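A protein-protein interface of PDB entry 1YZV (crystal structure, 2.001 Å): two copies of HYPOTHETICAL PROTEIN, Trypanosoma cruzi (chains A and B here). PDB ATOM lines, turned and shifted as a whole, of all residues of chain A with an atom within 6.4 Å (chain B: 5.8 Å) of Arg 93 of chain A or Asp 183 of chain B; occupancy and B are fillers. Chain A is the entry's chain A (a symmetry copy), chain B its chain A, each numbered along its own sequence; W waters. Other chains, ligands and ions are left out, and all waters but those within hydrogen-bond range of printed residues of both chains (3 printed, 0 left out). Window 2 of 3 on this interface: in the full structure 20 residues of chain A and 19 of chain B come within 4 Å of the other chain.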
ATOM      1  N   ASP A  27      -7.532  25.296 -18.752  1.00  0.00           N
ATOM      2  CA  ASP A  27      -8.295  24.491 -17.768  1.00  0.00           C
ATOM      3  C   ASP A  27      -7.938  24.748 -16.275  1.00  0.00           C
ATOM      4  O   ASP A  27      -7.844  23.814 -15.467  1.00  0.00           O
ATOM      5  CB  ASP A  27      -8.098  22.994 -18.090  1.00  0.00           C
ATOM      6  CG  ASP A  27      -8.569  22.599 -19.490  1.00  0.00           C
ATOM      7  OD1 ASP A  27      -9.061  23.462 -20.280  1.00  0.00           O
ATOM      8  OD2 ASP A  27      -8.222  21.442 -19.884  1.00  0.00           O
ATOM      9  N   GLN A  68     -12.209  22.168 -19.383  1.00  0.00           N
ATOM     10  CA  GLN A  68     -12.443  20.741 -19.605  1.00  0.00           C
ATOM     11  C   GLN A  68     -13.711  20.316 -18.878  1.00  0.00           C
ATOM     12  O   GLN A  68     -13.857  20.575 -17.684  1.00  0.00           O
ATOM     13  CB  GLN A  68     -11.287  19.908 -19.080  1.00  0.00           C
ATOM     14  CG  GLN A  68     -11.440  18.420 -19.243  1.00  0.00           C
ATOM     15  CD  GLN A  68     -11.190  17.938 -20.663  1.00  0.00           C
ATOM     16  OE1 GLN A  68     -10.670  18.687 -21.504  1.00  0.00           O
ATOM     17  NE2 GLN A  68     -11.473  16.651 -20.909  1.00  0.00           N
ATOM     18  N   LYS A  91     -14.436  22.058 -23.639  1.00  0.00           N
ATOM     19  CA  LYS A  91     -13.907  20.920 -24.413  1.00  0.00           C
ATOM     20  C   LYS A  91     -13.908  19.596 -23.623  1.00  0.00           C
ATOM     21  O   LYS A  91     -13.777  19.568 -22.403  1.00  0.00           O
ATOM     22  CB  LYS A  91     -12.466  21.189 -24.903  1.00  0.00           C
ATOM     23  CG  LYS A  91     -11.436  21.324 -23.719  1.00  0.00           C
ATOM     24  CD  LYS A  91     -10.065  21.780 -24.186  1.00  0.00           C
ATOM     25  CE  LYS A  91      -8.948  21.667 -23.110  1.00  0.00           C
ATOM     26  NZ  LYS A  91      -8.800  20.310 -22.476  1.00  0.00           N
ATOM     27  N   LYS A  92     -13.827  18.515 -24.389  1.00  0.00           N
ATOM     28  CA  LYS A  92     -13.484  17.200 -23.913  1.00  0.00           C
ATOM     29  C   LYS A  92     -12.145  16.721 -24.490  1.00  0.00           C
ATOM     30  O   LYS A  92     -11.515  15.873 -23.892  1.00  0.00           O
ATOM     31  CB  LYS A  92     -14.598  16.219 -24.253  1.00  0.00           C
ATOM     32  CG  LYS A  92     -15.883  16.564 -23.473  1.00  0.00           C
ATOM     33  CD  LYS A  92     -16.787  15.373 -23.343  1.00  0.00           C
ATOM     34  CE  LYS A  92     -18.097  15.745 -22.627  1.00  0.00           C
ATOM     35  NZ  LYS A  92     -18.967  16.614 -23.511  1.00  0.00           N
ATOM     36  N   ARG A  93     -11.700  17.286 -25.619  1.00  0.00           N
ATOM     37  CA  ARG A  93     -10.353  17.017 -26.144  1.00  0.00           C
ATOM     38  C   ARG A  93      -9.295  17.533 -25.145  1.00  0.00           C
ATOM     39  O   ARG A  93      -9.520  18.545 -24.464  1.00  0.00           O
ATOM     40  CB  ARG A  93     -10.170  17.698 -27.497  1.00  0.00           C
ATOM     41  CG  ARG A  93      -8.846  17.328 -28.207  1.00  0.00           C
ATOM     42  CD  ARG A  93      -8.534  18.218 -29.369  1.00  0.00           C
ATOM     43  NE  ARG A  93      -9.595  18.227 -30.359  1.00  0.00           N
ATOM     44  CZ  ARG A  93      -9.445  18.565 -31.638  1.00  0.00           C
ATOM     45  NH1 ARG A  93      -8.254  18.948 -32.121  1.00  0.00           N
ATOM     46  NH2 ARG A  93     -10.515  18.603 -32.416  1.00  0.00           N
ATOM     47  N   PHE A  94      -8.167  16.827 -24.988  1.00  0.00           N
ATOM     48  CA  PHE A  94      -7.200  17.265 -23.968  1.00  0.00           C
ATOM     49  C   PHE A  94      -6.451  18.500 -24.505  1.00  0.00           C
ATOM     50  O   PHE A  94      -6.436  19.554 -23.859  1.00  0.00           O
ATOM     51  CB  PHE A  94      -6.266  16.137 -23.555  1.00  0.00           C
ATOM     52  CG  PHE A  94      -6.977  14.964 -22.956  1.00  0.00           C
ATOM     53  CD1 PHE A  94      -8.024  15.150 -22.068  1.00  0.00           C
ATOM     54  CD2 PHE A  94      -6.634  13.686 -23.320  1.00  0.00           C
ATOM     55  CE1 PHE A  94      -8.725  14.067 -21.555  1.00  0.00           C
ATOM     56  CE2 PHE A  94      -7.234  12.590 -22.742  1.00  0.00           C
ATOM     57  CZ  PHE A  94      -8.346  12.784 -21.894  1.00  0.00           C
ATOM     58  N   ALA A  95      -5.990  18.417 -25.743  1.00  0.00           N
ATOM     59  CA  ALA A  95      -5.440  19.623 -26.439  1.00  0.00           C
ATOM     60  C   ALA A  95      -6.492  20.734 -26.633  1.00  0.00           C
ATOM     61  O   ALA A  95      -7.663  20.466 -26.912  1.00  0.00           O
ATOM     62  CB  ALA A  95      -4.819  19.242 -27.749  1.00  0.00           C
ATOM     63  N   MET A  96      -6.045  21.996 -26.559  1.00  0.00           N
ATOM     64  CA  MET A  96      -6.930  23.144 -26.602  1.00  0.00           C
ATOM     65  C   MET A  96      -7.368  23.482 -28.026  1.00  0.00           C
ATOM     66  O   MET A  96      -8.289  24.291 -28.182  1.00  0.00           O
ATOM     67  CB  MET A  96      -6.273  24.382 -25.987  1.00  0.00           C
ATOM     68  CG  MET A  96      -5.986  24.255 -24.511  1.00  0.00           C
ATOM     69  SD  MET A  96      -5.094  25.712 -23.922  1.00  0.00           S
ATOM     70  CE  MET A  96      -6.277  27.021 -24.185  1.00  0.00           C
ATOM     71  N   LEU A  97      -6.861  22.764 -29.032  1.00  0.00           N
ATOM     72  CA  LEU A  97      -7.009  23.199 -30.431  1.00  0.00           C
ATOM     73  C   LEU A  97      -8.262  22.650 -31.064  1.00  0.00           C
ATOM     74  O   LEU A  97      -8.235  21.966 -32.106  1.00  0.00           O
ATOM     75  CB  LEU A  97      -5.761  22.854 -31.263  1.00  0.00           C
ATOM     76  CG  LEU A  97      -4.548  23.714 -30.927  1.00  0.00           C
ATOM     77  CD1 LEU A  97      -3.399  23.202 -31.761  1.00  0.00           C
ATOM     78  CD2 LEU A  97      -4.813  25.171 -31.280  1.00  0.00           C
ATOM     79  N   VAL A  98      -9.361  22.919 -30.389  1.00  0.00           N
ATOM     80  CA  VAL A  98     -10.654  22.441 -30.812  1.00  0.00           C
ATOM     81  C   VAL A  98     -11.170  23.366 -31.918  1.00  0.00           C
ATOM     82  O   VAL A  98     -10.664  24.478 -32.088  1.00  0.00           O
ATOM     83  CB  VAL A  98     -11.609  22.332 -29.610  1.00  0.00           C
ATOM     84  CG1 VAL A  98     -11.080  21.271 -28.613  1.00  0.00           C
ATOM     85  CG2 VAL A  98     -11.768  23.663 -28.884  1.00  0.00           C
ATOM     86  N   PRO A  99     -12.138  22.889 -32.711  1.00  0.00           N
ATOM     87  CA  PRO A  99     -12.617  23.691 -33.863  1.00  0.00           C
ATOM     88  C   PRO A  99     -13.009  25.152 -33.571  1.00  0.00           C
ATOM     89  O   PRO A  99     -12.745  26.003 -34.384  1.00  0.00           O
ATOM     90  CB  PRO A  99     -13.814  22.888 -34.380  1.00  0.00           C
ATOM     91  CG  PRO A  99     -13.553  21.459 -33.948  1.00  0.00           C
ATOM     92  CD  PRO A  99     -12.765  21.542 -32.656  1.00  0.00           C
ATOM     93  N   CYS A 123      -3.306  18.176 -20.667  1.00  0.00           N
ATOM     94  CA  CYS A 123      -3.769  19.236 -21.564  1.00  0.00           C
ATOM     95  C   CYS A 123      -2.673  20.199 -22.047  1.00  0.00           C
ATOM     96  O   CYS A 123      -2.613  20.550 -23.229  1.00  0.00           O
ATOM     97  CB  CYS A 123      -5.006  19.933 -20.927  1.00  0.00           C
ATOM     98  SG  CYS A 123      -6.495  18.700 -20.752  1.00  0.00           S
ATOM     99  N   GLN A 126      -0.211  18.079 -24.498  1.00  0.00           N
ATOM    100  CA  GLN A 126      -0.866  17.805 -25.762  1.00  0.00           C
ATOM    101  C   GLN A 126      -1.173  19.060 -26.615  1.00  0.00           C
ATOM    102  O   GLN A 126      -1.131  19.005 -27.833  1.00  0.00           O
ATOM    103  CB  GLN A 126      -2.131  16.930 -25.581  1.00  0.00           C
ATOM    104  CG  GLN A 126      -1.781  15.606 -24.908  1.00  0.00           C
ATOM    105  CD  GLN A 126      -2.848  14.582 -24.944  1.00  0.00           C
ATOM    106  OE1 GLN A 126      -3.688  14.555 -25.867  1.00  0.00           O
ATOM    107  NE2 GLN A 126      -2.835  13.701 -23.940  1.00  0.00           N
ATOM    108  N   MET B 178      -3.215   9.098 -21.219  1.00  0.00           N
ATOM    109  CA  MET B 178      -3.982  10.208 -21.795  1.00  0.00           C
ATOM    110  C   MET B 178      -3.466  10.601 -23.190  1.00  0.00           C
ATOM    111  O   MET B 178      -4.253  11.030 -24.033  1.00  0.00           O
ATOM    112  CB  MET B 178      -3.975  11.398 -20.822  1.00  0.00           C
ATOM    113  CG  MET B 178      -4.623  11.067 -19.476  1.00  0.00           C
ATOM    114  SD  MET B 178      -6.361  10.703 -19.671  1.00  0.00           S
ATOM    115  CE  MET B 178      -6.432   8.917 -19.864  1.00  0.00           C
ATOM    116  N   LEU B 181      -5.299   8.124 -25.525  1.00  0.00           N
ATOM    117  CA  LEU B 181      -6.724   8.436 -25.648  1.00  0.00           C
ATOM    118  C   LEU B 181      -7.090   9.766 -26.298  1.00  0.00           C
ATOM    119  O   LEU B 181      -8.160   9.865 -26.918  1.00  0.00           O
ATOM    120  CB  LEU B 181      -7.427   8.344 -24.300  1.00  0.00           C
ATOM    121  CG  LEU B 181      -7.949   6.971 -23.874  1.00  0.00           C
ATOM    122  CD1 LEU B 181      -6.893   5.874 -23.962  1.00  0.00           C
ATOM    123  CD2 LEU B 181      -8.365   7.124 -22.491  1.00  0.00           C
ATOM    124  N   LYS B 182      -6.356  10.824 -25.957  1.00  0.00           N
ATOM    125  CA  LYS B 182      -6.502  12.173 -26.553  1.00  0.00           C
ATOM    126  C   LYS B 182      -7.733  13.035 -26.230  1.00  0.00           C
ATOM    127  O   LYS B 182      -7.644  14.269 -26.338  1.00  0.00           O
ATOM    128  CB  LYS B 182      -6.258  12.169 -28.084  1.00  0.00           C
ATOM    129  CG  LYS B 182      -4.879  11.529 -28.403  1.00  0.00           C
ATOM    130  CD  LYS B 182      -4.129  12.124 -29.544  1.00  0.00           C
ATOM    131  CE  LYS B 182      -2.693  11.473 -29.686  1.00  0.00           C
ATOM    132  NZ  LYS B 182      -1.598  11.617 -28.565  1.00  0.00           N
ATOM    133  N   ASP B 183      -8.805  12.435 -25.729  1.00  0.00           N
ATOM    134  CA  ASP B 183     -10.080  13.100 -25.616  1.00  0.00           C
ATOM    135  C   ASP B 183     -10.967  12.300 -24.630  1.00  0.00           C
ATOM    136  O   ASP B 183     -11.064  11.072 -24.717  1.00  0.00           O
ATOM    137  CB  ASP B 183     -10.668  13.220 -27.054  1.00  0.00           C
ATOM    138  CG  ASP B 183     -11.923  14.070 -27.142  1.00  0.00           C
ATOM    139  OD1 ASP B 183     -12.847  13.907 -26.311  1.00  0.00           O
ATOM    140  OD2 ASP B 183     -12.055  14.790 -28.155  1.00  0.00           O
ATOM    141  N   ALA B 184     -11.592  12.991 -23.667  1.00  0.00           N
ATOM    142  CA  ALA B 184     -12.473  12.343 -22.710  1.00  0.00           C
ATOM    143  C   ALA B 184     -13.716  11.748 -23.314  1.00  0.00           C
ATOM    144  O   ALA B 184     -14.418  10.986 -22.633  1.00  0.00           O
ATOM    145  CB  ALA B 184     -12.879  13.334 -21.571  1.00  0.00           C
ATOM    146  N   SER B 185     -14.063  12.148 -24.532  1.00  0.00           N
ATOM    147  CA  SER B 185     -15.211  11.551 -25.190  1.00  0.00           C
ATOM    148  C   SER B 185     -14.856  10.291 -25.964  1.00  0.00           C
ATOM    149  O   SER B 185     -15.735   9.650 -26.529  1.00  0.00           O
ATOM    150  CB  SER B 185     -15.912  12.557 -26.099  1.00  0.00           C
ATOM    151  OG  SER B 185     -15.216  12.716 -27.314  1.00  0.00           O
ATOM    152  N   ASP B 186     -13.585   9.911 -25.984  1.00  0.00           N
ATOM    153  CA  ASP B 186     -13.200   8.641 -26.564  1.00  0.00           C
ATOM    154  C   ASP B 186     -13.982   7.468 -25.943  1.00  0.00           C
ATOM    155  O   ASP B 186     -14.208   7.433 -24.733  1.00  0.00           O
ATOM    156  CB  ASP B 186     -11.700   8.398 -26.432  1.00  0.00           C
ATOM    157  CG  ASP B 186     -11.260   7.142 -27.171  1.00  0.00           C
ATOM    158  OD1 ASP B 186     -11.386   6.014 -26.610  1.00  0.00           O
ATOM    159  OD2 ASP B 186     -10.740   7.276 -28.284  1.00  0.00           O
ATOM    160  N   PHE B 189     -12.570   5.961 -22.698  1.00  0.00           N
ATOM    161  CA  PHE B 189     -12.214   6.795 -21.555  1.00  0.00           C
ATOM    162  C   PHE B 189     -12.883   6.373 -20.239  1.00  0.00           C
ATOM    163  O   PHE B 189     -12.229   6.279 -19.166  1.00  0.00           O
ATOM    164  CB  PHE B 189     -12.499   8.272 -21.818  1.00  0.00           C
ATOM    165  CG  PHE B 189     -12.034   9.149 -20.721  1.00  0.00           C
ATOM    166  CD1 PHE B 189     -10.700   9.492 -20.611  1.00  0.00           C
ATOM    167  CD2 PHE B 189     -12.935   9.674 -19.802  1.00  0.00           C
ATOM    168  CE1 PHE B 189     -10.260  10.304 -19.554  1.00  0.00           C
ATOM    169  CE2 PHE B 189     -12.498  10.441 -18.772  1.00  0.00           C
ATOM    170  CZ  PHE B 189     -11.158  10.791 -18.673  1.00  0.00           C
HETATM  171  O   HOH W   1      -1.471  14.492 -28.329  1.00  0.00           O
HETATM  172  O   HOH W   2      -5.707  15.905 -27.222  1.00  0.00           O
HETATM  173  O   HOH W   3     -10.626  15.228 -30.288  1.00  0.00           O
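The side-chain amide nitrogen (NE2) of Gln 126 of chain A lies within hydrogen-bond range of the backbone carbonyl oxygen (O) of Met 178 of chain B, at 3.0 Å. O of Lys 182 of chain B is in hydrogen-bond range of N of Phe 94 of chain A (2.9 Å). The backbone NH (N) of Ala 184 of chain B lies within hydrogen-bond range of the backbone carbonyl oxygen (O) of Lys 92 of chain A (2.9 Å). The backbone carbonyl oxygen (O) of Lys 92 of chain A sits close to the side-chain carboxylate (OD1) of Asp 183 of chain B (3.4 Å).
Water W3 lies within hydrogen-bond range of OD2 of Asp 183 of chain B and NE of Arg 93 of chain A. Water W2 lies within hydrogen-bond range of O of Lys 182 of chain B, OE1 of Gln 126 of chain A, N of Ala 95 of chain A and N of Phe 94 of chain A. Water W1 bridges NZ of Lys 182 of chain B (2.9 Å) and OE1 of Gln 126 of chain A (3.3 Å).
Ala 184 of chain B touches Gln 68 of chain A (CB to NE2, 3.7 Å). CG of Arg 93 of chain A touches O of Lys 182 of chain B, at 3.8 Å. Arg 93 of chain A touches Asp 183 of chain B. Phe 94 of chain A touches Met 178 of chain B. Asp 183 of chain B touches Phe 94 of chain A (N to CE2, 3.4 Å). Ala 184 of chain B touches Phe 94 of chain A (N to CZ, 3.7 Å). CZ of Phe 94 of chain A touches CE1 of Phe 189 of chain B (3.9 Å). OE1 of Gln 126 of chain A touches CA of Lys 182 of chain B, at 3.8 Å.
Printed residues of chain B within 4 Å of Arg 93 of chain A: Lys 182 (3.8 Å) and Asp 183 (3.4 Å). Printed residues of chain A within 4 Å of Asp 183 of chain B: Lys 92, Arg 93 and Phe 94. Of the printed residues of chain B, Gln 68 of chain A touches Ala 184. Of the printed residues of chain B, Gln 126 of chain A touches Met 178 and Lys 182. Of the printed residues of chain B, Lys 92 of chain A touches Asp 183 and Ala 184. Printed residues of chain A within 4 Å of Ala 184 of chain B: Gln 68, Lys 92 and Phe 94. The nearest residue of chain B that does not touch Arg 93 of chain A is Ala 184 of chain B (4.7 Å). The nearest residue of chain A that does not touch Asp 183 of chain B is Gln 126 of chain A (5.5 Å).
Printed residues of chain B that touch a printed residue of chain A: Met 178, Lys 182, Asp 183, Ala 184 and Phe 189. Hydrophobic or aromatic side chains of chain B that line the printed part of chain A: Met 178, Ala 184 and Phe 189. Printed residues of chain A that touch a printed residue of chain B: Gln 68, Lys 92, Arg 93, Phe 94 and Gln 126. Hydrophobic or aromatic side chains of chain A within 4 Å of the printed part of chain B: Phe 94. Among the printed residues, 12 pairs touch across the chains. Among the printed residues, no Asp or Glu carboxylate lies within 4 Å of a Lys or Arg side-chain nitrogen of the other chain.
OD1 of Asp 183 of chain B is in hydrogen-bond range of N of Ser 185 of chain B (2.8 Å). OE1 of Gln 68 of chain A is in hydrogen-bond range of NZ of Lys 91 of chain A, 2.7 Å away. NE2 of Gln 68 of chain A lies within hydrogen-bond range of O of Lys 92 of chain A. OE1 of Gln 68 of chain A lies close to O of Arg 93 of chain A. NH1 of Arg 93 of chain A lies within hydrogen-bond range of O of Leu 97 of chain A (3.0 Å). The backbone carbonyl oxygen (O) of Phe 94 of chain A sits at hydrogen-bond distance from the side-chain sulfur (SG) of Cys 123 of chain A.
No position is printed for both chains.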
